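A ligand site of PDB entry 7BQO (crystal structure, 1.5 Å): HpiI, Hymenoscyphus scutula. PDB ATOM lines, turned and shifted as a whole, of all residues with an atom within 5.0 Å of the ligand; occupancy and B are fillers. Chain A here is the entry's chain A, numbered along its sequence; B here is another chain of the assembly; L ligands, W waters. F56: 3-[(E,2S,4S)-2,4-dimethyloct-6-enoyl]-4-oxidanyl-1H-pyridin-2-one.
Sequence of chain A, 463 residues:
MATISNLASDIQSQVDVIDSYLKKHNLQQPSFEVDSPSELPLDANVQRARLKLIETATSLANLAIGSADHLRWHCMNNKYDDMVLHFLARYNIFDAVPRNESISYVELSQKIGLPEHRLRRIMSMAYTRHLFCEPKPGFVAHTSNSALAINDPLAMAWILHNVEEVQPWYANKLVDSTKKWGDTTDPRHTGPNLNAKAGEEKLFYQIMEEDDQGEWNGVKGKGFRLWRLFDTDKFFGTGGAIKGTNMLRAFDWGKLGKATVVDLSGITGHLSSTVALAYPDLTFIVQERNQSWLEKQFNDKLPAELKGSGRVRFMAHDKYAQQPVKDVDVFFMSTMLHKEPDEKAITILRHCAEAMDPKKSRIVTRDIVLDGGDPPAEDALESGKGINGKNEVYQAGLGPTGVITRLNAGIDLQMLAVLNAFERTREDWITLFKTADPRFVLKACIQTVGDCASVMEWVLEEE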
ATOM      1  N   TRP A 158     -35.298 -29.003   3.464  1.00  0.00           N
ATOM      2  CA  TRP A 158     -33.935 -29.549   3.446  1.00  0.00           C
ATOM      3  C   TRP A 158     -33.423 -29.702   2.013  1.00  0.00           C
ATOM      4  O   TRP A 158     -32.268 -29.386   1.731  1.00  0.00           O
ATOM      5  CB  TRP A 158     -33.979 -30.892   4.170  1.00  0.00           C
ATOM      6  CG  TRP A 158     -32.586 -31.514   4.320  1.00  0.00           C
ATOM      7  CD1 TRP A 158     -32.299 -32.820   4.024  1.00  0.00           C
ATOM      8  CD2 TRP A 158     -31.409 -30.924   4.900  1.00  0.00           C
ATOM      9  NE1 TRP A 158     -30.943 -33.072   4.307  1.00  0.00           N
ATOM     10  CE2 TRP A 158     -30.411 -31.928   4.878  1.00  0.00           C
ATOM     11  CE3 TRP A 158     -31.091 -29.649   5.427  1.00  0.00           C
ATOM     12  CZ2 TRP A 158     -29.105 -31.704   5.310  1.00  0.00           C
ATOM     13  CZ3 TRP A 158     -29.813 -29.434   5.904  1.00  0.00           C
ATOM     14  CH2 TRP A 158     -28.836 -30.472   5.865  1.00  0.00           C
ATOM     15  N   HIS A 161     -32.819 -25.875   0.792  1.00  0.00           N
ATOM     16  CA  HIS A 161     -31.663 -25.215   1.409  1.00  0.00           C
ATOM     17  C   HIS A 161     -30.358 -25.725   0.805  1.00  0.00           C
ATOM     18  O   HIS A 161     -29.453 -24.931   0.508  1.00  0.00           O
ATOM     19  CB  HIS A 161     -31.668 -25.470   2.928  1.00  0.00           C
ATOM     20  CG  HIS A 161     -30.412 -25.050   3.633  1.00  0.00           C
ATOM     21  ND1 HIS A 161     -29.893 -23.775   3.504  1.00  0.00           N
ATOM     22  CD2 HIS A 161     -29.603 -25.718   4.488  1.00  0.00           C
ATOM     23  CE1 HIS A 161     -28.799 -23.697   4.256  1.00  0.00           C
ATOM     24  NE2 HIS A 161     -28.614 -24.857   4.876  1.00  0.00           N
ATOM     25  N   VAL A 166     -26.790 -23.836  -0.083  1.00  0.00           N
ATOM     26  CA  VAL A 166     -25.478 -24.343   0.336  1.00  0.00           C
ATOM     27  C   VAL A 166     -24.618 -24.675  -0.877  1.00  0.00           C
ATOM     28  O   VAL A 166     -23.465 -24.234  -0.967  1.00  0.00           O
ATOM     29  CB  VAL A 166     -25.649 -25.588   1.209  1.00  0.00           C
ATOM     30  CG1 VAL A 166     -24.234 -26.150   1.578  1.00  0.00           C
ATOM     31  CG2 VAL A 166     -26.500 -25.225   2.466  1.00  0.00           C
ATOM     32  N   PHE A 204     -23.667 -15.699   6.137  1.00  0.00           N
ATOM     33  CA  PHE A 204     -24.810 -16.577   5.834  1.00  0.00           C
ATOM     34  C   PHE A 204     -26.028 -16.205   6.663  1.00  0.00           C
ATOM     35  O   PHE A 204     -27.152 -16.100   6.124  1.00  0.00           O
ATOM     36  CB  PHE A 204     -24.392 -18.040   6.099  1.00  0.00           C
ATOM     37  CG  PHE A 204     -25.566 -18.998   6.120  1.00  0.00           C
ATOM     38  CD1 PHE A 204     -26.171 -19.396   4.929  1.00  0.00           C
ATOM     39  CD2 PHE A 204     -26.029 -19.474   7.359  1.00  0.00           C
ATOM     40  CE1 PHE A 204     -27.258 -20.289   4.935  1.00  0.00           C
ATOM     41  CE2 PHE A 204     -27.144 -20.332   7.423  1.00  0.00           C
ATOM     42  CZ  PHE A 204     -27.707 -20.754   6.178  1.00  0.00           C
ATOM     43  N   TYR A 205     -25.850 -16.038   7.990  1.00  0.00           N
ATOM     44  CA  TYR A 205     -27.042 -15.781   8.811  1.00  0.00           C
ATOM     45  C   TYR A 205     -27.618 -14.394   8.546  1.00  0.00           C
ATOM     46  O   TYR A 205     -28.815 -14.177   8.777  1.00  0.00           O
ATOM     47  CB  TYR A 205     -26.684 -15.972  10.308  1.00  0.00           C
ATOM     48  CG  TYR A 205     -26.914 -17.414  10.699  1.00  0.00           C
ATOM     49  CD1 TYR A 205     -28.206 -17.887  10.947  1.00  0.00           C
ATOM     50  CD2 TYR A 205     -25.847 -18.352  10.756  1.00  0.00           C
ATOM     51  CE1 TYR A 205     -28.467 -19.210  11.270  1.00  0.00           C
ATOM     52  CE2 TYR A 205     -26.109 -19.675  11.080  1.00  0.00           C
ATOM     53  CZ  TYR A 205     -27.405 -20.106  11.332  1.00  0.00           C
ATOM     54  OH  TYR A 205     -27.673 -21.423  11.635  1.00  0.00           O
ATOM     55  N   LEU A 229     -34.688 -22.436   7.030  1.00  0.00           N
ATOM     56  CA  LEU A 229     -33.589 -23.106   7.740  1.00  0.00           C
ATOM     57  C   LEU A 229     -34.106 -23.708   9.049  1.00  0.00           C
ATOM     58  O   LEU A 229     -33.688 -24.815   9.436  1.00  0.00           O
ATOM     59  CB  LEU A 229     -32.455 -22.090   7.974  1.00  0.00           C
ATOM     60  CG  LEU A 229     -31.231 -22.762   8.560  1.00  0.00           C
ATOM     61  CD1 LEU A 229     -30.536 -23.749   7.603  1.00  0.00           C
ATOM     62  CD2 LEU A 229     -30.243 -21.653   8.951  1.00  0.00           C
ATOM     63  N   THR A 232     -35.578 -26.934   8.414  1.00  0.00           N
ATOM     64  CA  THR A 232     -34.606 -27.987   8.216  1.00  0.00           C
ATOM     65  C   THR A 232     -34.115 -28.554   9.521  1.00  0.00           C
ATOM     66  O   THR A 232     -33.866 -29.707   9.634  1.00  0.00           O
ATOM     67  CB  THR A 232     -33.394 -27.596   7.360  1.00  0.00           C
ATOM     68  OG1 THR A 232     -32.521 -26.749   8.080  1.00  0.00           O
ATOM     69  CG2 THR A 232     -33.827 -26.949   6.103  1.00  0.00           C
ATOM     70  N   ASP A 233     -33.948 -27.666  10.494  1.00  0.00           N
ATOM     71  CA  ASP A 233     -33.495 -28.143  11.784  1.00  0.00           C
ATOM     72  C   ASP A 233     -34.537 -29.060  12.422  1.00  0.00           C
ATOM     73  O   ASP A 233     -34.200 -30.147  12.935  1.00  0.00           O
ATOM     74  CB  ASP A 233     -33.231 -26.913  12.648  1.00  0.00           C
ATOM     75  CG  ASP A 233     -32.519 -27.267  13.933  1.00  0.00           C
ATOM     76  OD1 ASP A 233     -31.275 -27.496  13.839  1.00  0.00           O
ATOM     77  OD2 ASP A 233     -33.184 -27.355  14.994  1.00  0.00           O
ATOM     78  N   PHE A 236     -34.532 -32.655  11.110  1.00  0.00           N
ATOM     79  CA  PHE A 236     -33.638 -33.636  11.680  1.00  0.00           C
ATOM     80  C   PHE A 236     -34.049 -34.112  13.063  1.00  0.00           C
ATOM     81  O   PHE A 236     -33.523 -35.121  13.541  1.00  0.00           O
ATOM     82  CB  PHE A 236     -32.205 -33.092  11.679  1.00  0.00           C
ATOM     83  CG  PHE A 236     -31.547 -33.321  10.348  1.00  0.00           C
ATOM     84  CD1 PHE A 236     -31.785 -32.467   9.267  1.00  0.00           C
ATOM     85  CD2 PHE A 236     -30.789 -34.468  10.154  1.00  0.00           C
ATOM     86  CE1 PHE A 236     -31.301 -32.727   7.999  1.00  0.00           C
ATOM     87  CE2 PHE A 236     -30.215 -34.706   8.858  1.00  0.00           C
ATOM     88  CZ  PHE A 236     -30.479 -33.823   7.813  1.00  0.00           C
ATOM     89  N   ILE A 242     -30.933 -38.602  13.839  1.00  0.00           N
ATOM     90  CA  ILE A 242     -30.740 -37.611  14.911  1.00  0.00           C
ATOM     91  C   ILE A 242     -32.063 -37.271  15.580  1.00  0.00           C
ATOM     92  O   ILE A 242     -32.188 -36.197  16.190  1.00  0.00           O
ATOM     93  CB  ILE A 242     -30.043 -36.328  14.384  1.00  0.00           C
ATOM     94  CG1 ILE A 242     -29.060 -36.669  13.247  1.00  0.00           C
ATOM     95  CG2 ILE A 242     -29.285 -35.682  15.562  1.00  0.00           C
ATOM     96  CD1 ILE A 242     -28.251 -35.423  12.804  1.00  0.00           C
ATOM     97  N   THR A 335     -26.998 -29.145  19.306  1.00  0.00           N
ATOM     98  CA  THR A 335     -26.461 -28.793  17.987  1.00  0.00           C
ATOM     99  C   THR A 335     -26.387 -27.287  17.763  1.00  0.00           C
ATOM    100  O   THR A 335     -26.726 -26.741  16.709  1.00  0.00           O
ATOM    101  CB  THR A 335     -27.183 -29.502  16.809  1.00  0.00           C
ATOM    102  OG1 THR A 335     -28.469 -28.943  16.533  1.00  0.00           O
ATOM    103  CG2 THR A 335     -27.328 -30.956  17.115  1.00  0.00           C
ATOM    104  N   HIS A 338     -21.655 -26.518  17.971  1.00  0.00           N
ATOM    105  CA  HIS A 338     -20.821 -26.916  16.826  1.00  0.00           C
ATOM    106  C   HIS A 338     -20.718 -25.811  15.779  1.00  0.00           C
ATOM    107  O   HIS A 338     -19.806 -25.875  14.949  1.00  0.00           O
ATOM    108  CB  HIS A 338     -21.306 -28.266  16.214  1.00  0.00           C
ATOM    109  CG  HIS A 338     -22.566 -28.169  15.391  1.00  0.00           C
ATOM    110  ND1 HIS A 338     -22.632 -28.741  14.150  1.00  0.00           N
ATOM    111  CD2 HIS A 338     -23.792 -27.586  15.601  1.00  0.00           C
ATOM    112  CE1 HIS A 338     -23.842 -28.570  13.620  1.00  0.00           C
ATOM    113  NE2 HIS A 338     -24.553 -27.824  14.459  1.00  0.00           N
ATOM    114  N   LYS A 339     -21.592 -24.794  15.783  1.00  0.00           N
ATOM    115  CA  LYS A 339     -21.479 -23.674  14.849  1.00  0.00           C
ATOM    116  C   LYS A 339     -20.535 -22.569  15.357  1.00  0.00           C
ATOM    117  O   LYS A 339     -20.435 -21.529  14.707  1.00  0.00           O
ATOM    118  CB  LYS A 339     -22.879 -23.098  14.635  1.00  0.00           C
ATOM    119  CG  LYS A 339     -23.797 -24.092  13.986  1.00  0.00           C
ATOM    120  CD  LYS A 339     -25.197 -23.308  13.827  1.00  0.00           C
ATOM    121  CE  LYS A 339     -26.233 -23.686  14.721  1.00  0.00           C
ATOM    122  NZ  LYS A 339     -27.355 -22.717  14.383  1.00  0.00           N
ATOM    123  N   ILE A 368     -22.132 -33.708  17.696  1.00  0.00           N
ATOM    124  CA  ILE A 368     -21.235 -34.737  17.226  1.00  0.00           C
ATOM    125  C   ILE A 368     -19.988 -34.804  18.092  1.00  0.00           C
ATOM    126  O   ILE A 368     -19.376 -33.773  18.447  1.00  0.00           O
ATOM    127  CB  ILE A 368     -20.855 -34.438  15.783  1.00  0.00           C
ATOM    128  CG1 ILE A 368     -22.049 -34.726  14.851  1.00  0.00           C
ATOM    129  CG2 ILE A 368     -19.605 -35.317  15.353  1.00  0.00           C
ATOM    130  CD1 ILE A 368     -21.773 -34.192  13.431  1.00  0.00           C
ATOM    131  N   ILE A 411     -21.831 -33.270   7.679  1.00  0.00           N
ATOM    132  CA  ILE A 411     -22.164 -32.160   8.558  1.00  0.00           C
ATOM    133  C   ILE A 411     -20.950 -31.251   8.784  1.00  0.00           C
ATOM    134  O   ILE A 411     -21.076 -30.011   8.715  1.00  0.00           O
ATOM    135  CB  ILE A 411     -22.714 -32.726   9.883  1.00  0.00           C
ATOM    136  CG1 ILE A 411     -24.073 -33.427   9.604  1.00  0.00           C
ATOM    137  CG2 ILE A 411     -22.850 -31.605  10.979  1.00  0.00           C
ATOM    138  CD1 ILE A 411     -24.461 -34.321  10.772  1.00  0.00           C
ATOM    139  N   GLN A 414     -20.436 -29.118   5.790  1.00  0.00           N
ATOM    140  CA  GLN A 414     -21.440 -28.056   5.748  1.00  0.00           C
ATOM    141  C   GLN A 414     -21.043 -26.937   6.692  1.00  0.00           C
ATOM    142  O   GLN A 414     -21.178 -25.763   6.324  1.00  0.00           O
ATOM    143  CB  GLN A 414     -22.806 -28.638   6.091  1.00  0.00           C
ATOM    144  CG  GLN A 414     -24.001 -27.703   5.680  1.00  0.00           C
ATOM    145  CD  GLN A 414     -24.888 -28.340   4.615  1.00  0.00           C
ATOM    146  OE1 GLN A 414     -24.405 -28.930   3.657  1.00  0.00           O
ATOM    147  NE2 GLN A 414     -26.192 -28.246   4.826  1.00  0.00           N
ATOM    148  N   MET A 415     -20.564 -27.281   7.890  1.00  0.00           N
ATOM    149  CA  MET A 415     -20.083 -26.254   8.800  1.00  0.00           C
ATOM    150  C   MET A 415     -18.913 -25.475   8.207  1.00  0.00           C
ATOM    151  O   MET A 415     -18.856 -24.242   8.320  1.00  0.00           O
ATOM    152  CB  MET A 415     -19.659 -26.862  10.140  1.00  0.00           C
ATOM    153  CG  MET A 415     -20.784 -27.481  10.955  1.00  0.00           C
ATOM    154  SD  MET A 415     -21.919 -26.153  11.530  1.00  0.00           S
ATOM    155  CE  MET A 415     -23.116 -26.364  10.300  1.00  0.00           C
ATOM    156  N   VAL A 418     -20.334 -23.263   4.983  1.00  0.00           N
ATOM    157  CA  VAL A 418     -21.284 -22.189   5.234  1.00  0.00           C
ATOM    158  C   VAL A 418     -20.744 -21.200   6.260  1.00  0.00           C
ATOM    159  O   VAL A 418     -21.036 -20.021   6.169  1.00  0.00           O
ATOM    160  CB  VAL A 418     -22.604 -22.810   5.688  1.00  0.00           C
ATOM    161  CG1 VAL A 418     -23.712 -21.709   5.939  1.00  0.00           C
ATOM    162  CG2 VAL A 418     -23.132 -23.677   4.566  1.00  0.00           C
ATOM    163  N   LEU A 419     -19.963 -21.691   7.219  1.00  0.00           N
ATOM    164  CA  LEU A 419     -19.636 -20.905   8.402  1.00  0.00           C
ATOM    165  C   LEU A 419     -18.140 -20.825   8.726  1.00  0.00           C
ATOM    166  O   LEU A 419     -17.772 -20.023   9.573  1.00  0.00           O
ATOM    167  CB  LEU A 419     -20.354 -21.428   9.663  1.00  0.00           C
ATOM    168  CG  LEU A 419     -21.897 -21.432   9.626  1.00  0.00           C
ATOM    169  CD1 LEU A 419     -22.441 -22.106  10.883  1.00  0.00           C
ATOM    170  CD2 LEU A 419     -22.452 -19.993   9.462  1.00  0.00           C
ATOM    171  N   CYS A 452     -25.634 -39.803  15.093  1.00  0.00           N
ATOM    172  CA  CYS A 452     -24.313 -39.227  15.041  1.00  0.00           C
ATOM    173  C   CYS A 452     -23.978 -38.335  16.243  1.00  0.00           C
ATOM    174  O   CYS A 452     -22.783 -37.989  16.419  1.00  0.00           O
ATOM    175  CB  CYS A 452     -24.064 -38.451  13.734  1.00  0.00           C
ATOM    176  SG  CYS A 452     -25.192 -37.050  13.537  1.00  0.00           S
ATOM    177  N   MET B  76     -27.613 -34.058   2.769  1.00  0.00           N
ATOM    178  CA  MET B  76     -26.382 -33.715   3.490  1.00  0.00           C
ATOM    179  C   MET B  76     -25.103 -34.064   2.730  1.00  0.00           C
ATOM    180  O   MET B  76     -24.194 -33.222   2.607  1.00  0.00           O
ATOM    181  CB  MET B  76     -26.382 -34.463   4.826  1.00  0.00           C
ATOM    182  CG  MET B  76     -25.293 -33.966   5.754  1.00  0.00           C
ATOM    183  SD  MET B  76     -25.704 -32.374   6.529  1.00  0.00           S
ATOM    184  CE  MET B  76     -26.930 -32.909   7.748  1.00  0.00           C
HETATM  185  C1  F56 L   1     -26.599 -24.028   9.233  1.00  0.00           C
HETATM  186  C2  F56 L   1     -26.948 -24.083   7.872  1.00  0.00           C
HETATM  187  C4  F56 L   1     -27.127 -26.471   7.939  1.00  0.00           C
HETATM  188  C5  F56 L   1     -26.742 -26.449   9.293  1.00  0.00           C
HETATM  189  C6  F56 L   1     -26.559 -25.212   9.902  1.00  0.00           C
HETATM  190  C7  F56 L   1     -26.553 -27.688  10.156  1.00  0.00           C
HETATM  191  C8  F56 L   1     -26.622 -29.068   9.522  1.00  0.00           C
HETATM  192  C9  F56 L   1     -26.783 -30.174  10.559  1.00  0.00           C
HETATM  193  C10 F56 L   1     -28.127 -30.154  11.303  1.00  0.00           C
HETATM  194  C11 F56 L   1     -28.210 -31.337  12.282  1.00  0.00           C
HETATM  195  C12 F56 L   1     -27.123 -31.282  13.347  1.00  0.00           C
HETATM  196  C13 F56 L   1     -26.290 -32.256  13.480  1.00  0.00           C
HETATM  197  C14 F56 L   1     -25.177 -32.303  14.503  1.00  0.00           C
HETATM  198  C18 F56 L   1     -25.267 -29.272   8.780  1.00  0.00           C
HETATM  199  C19 F56 L   1     -29.331 -30.356  10.346  1.00  0.00           C
HETATM  200  N3  F56 L   1     -27.130 -25.281   7.253  1.00  0.00           N
HETATM  201  O15 F56 L   1     -26.218 -25.161  11.245  1.00  0.00           O
HETATM  202  O16 F56 L   1     -26.168 -27.598  11.310  1.00  0.00           O
HETATM  203  O17 F56 L   1     -27.350 -27.508   7.303  1.00  0.00           O
HETATM  204  O   HOH W   1     -22.628 -31.278  16.428  1.00  0.00           O
HETATM  205  O   HOH W   2     -29.984 -27.183   9.114  1.00  0.00           O
HETATM  206  O   HOH W   3     -27.138 -27.194  13.883  1.00  0.00           O
HETATM  207  O   HOH W   4     -29.439 -26.709  11.830  1.00  0.00           O
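Water W3 lies within hydrogen-bond range of NE2 of His 338 (2.7 Å), O16 of the ligand (2.8 Å) and O of Thr 335 (2.9 Å). Water W2 lies within hydrogen-bond range of the side-chain hydroxyl of Thr 232 (2.8 Å) and an oxygen (O17) of the ligand (3.2 Å). Water W1 lies within hydrogen-bond range of the backbone NH of Ile 368 (2.8 Å) and a ring nitrogen (ND1) of His 338 (3.4 Å). Water W4 bridges the side-chain carboxylate of Asp 233 (2.8 Å) and an oxygen (O16) of the ligand (3.4 Å).
The backbone carbonyl oxygen of His 161 lies within hydrogen-bond range of the backbone NH of Val 166 (2.9 Å). The side-chain amino group (NZ) of Lys 339 lies within hydrogen-bond range of the side-chain hydroxyl (OH) of Tyr 205 (3.1 Å). A ring nitrogen (ND1) of His 338 lies close to the side-chain sulfur (SD) of Met 415, 3.8 Å away. A ring nitrogen (NE2) of His 338 sits close to the backbone carbonyl oxygen of Thr 335 (3.3 Å). The side-chain hydroxyl (OG1) of Thr 232 is in hydrogen-bond range of the backbone carbonyl oxygen (O) of Leu 229 (2.6 Å).
The side-chain amide nitrogen (NE2) of Gln 414 sits at hydrogen-bond distance from an oxygen (O17) of the ligand, 2.8 Å away. A nitrogen (N3) of the ligand sits at hydrogen-bond distance from a ring nitrogen (NE2) of His 161 (2.8 Å).
Residues that only touch the ligand: Lys 339, Phe 236, His 338, Trp 158, Met 415, Leu 229, Thr 335, Tyr 205, Phe 204, Ile 242, Met 76 of chain B, Ile 411 and Ile 368. 15 residues have an atom within 4 Å of the ligand: Trp 158, His 161, Phe 204, Tyr 205, Leu 229, Phe 236, Ile 242, Thr 335, His 338, Lys 339, Ile 368, Ile 411, Gln 414, Met 415 and Met 76 of chain B.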
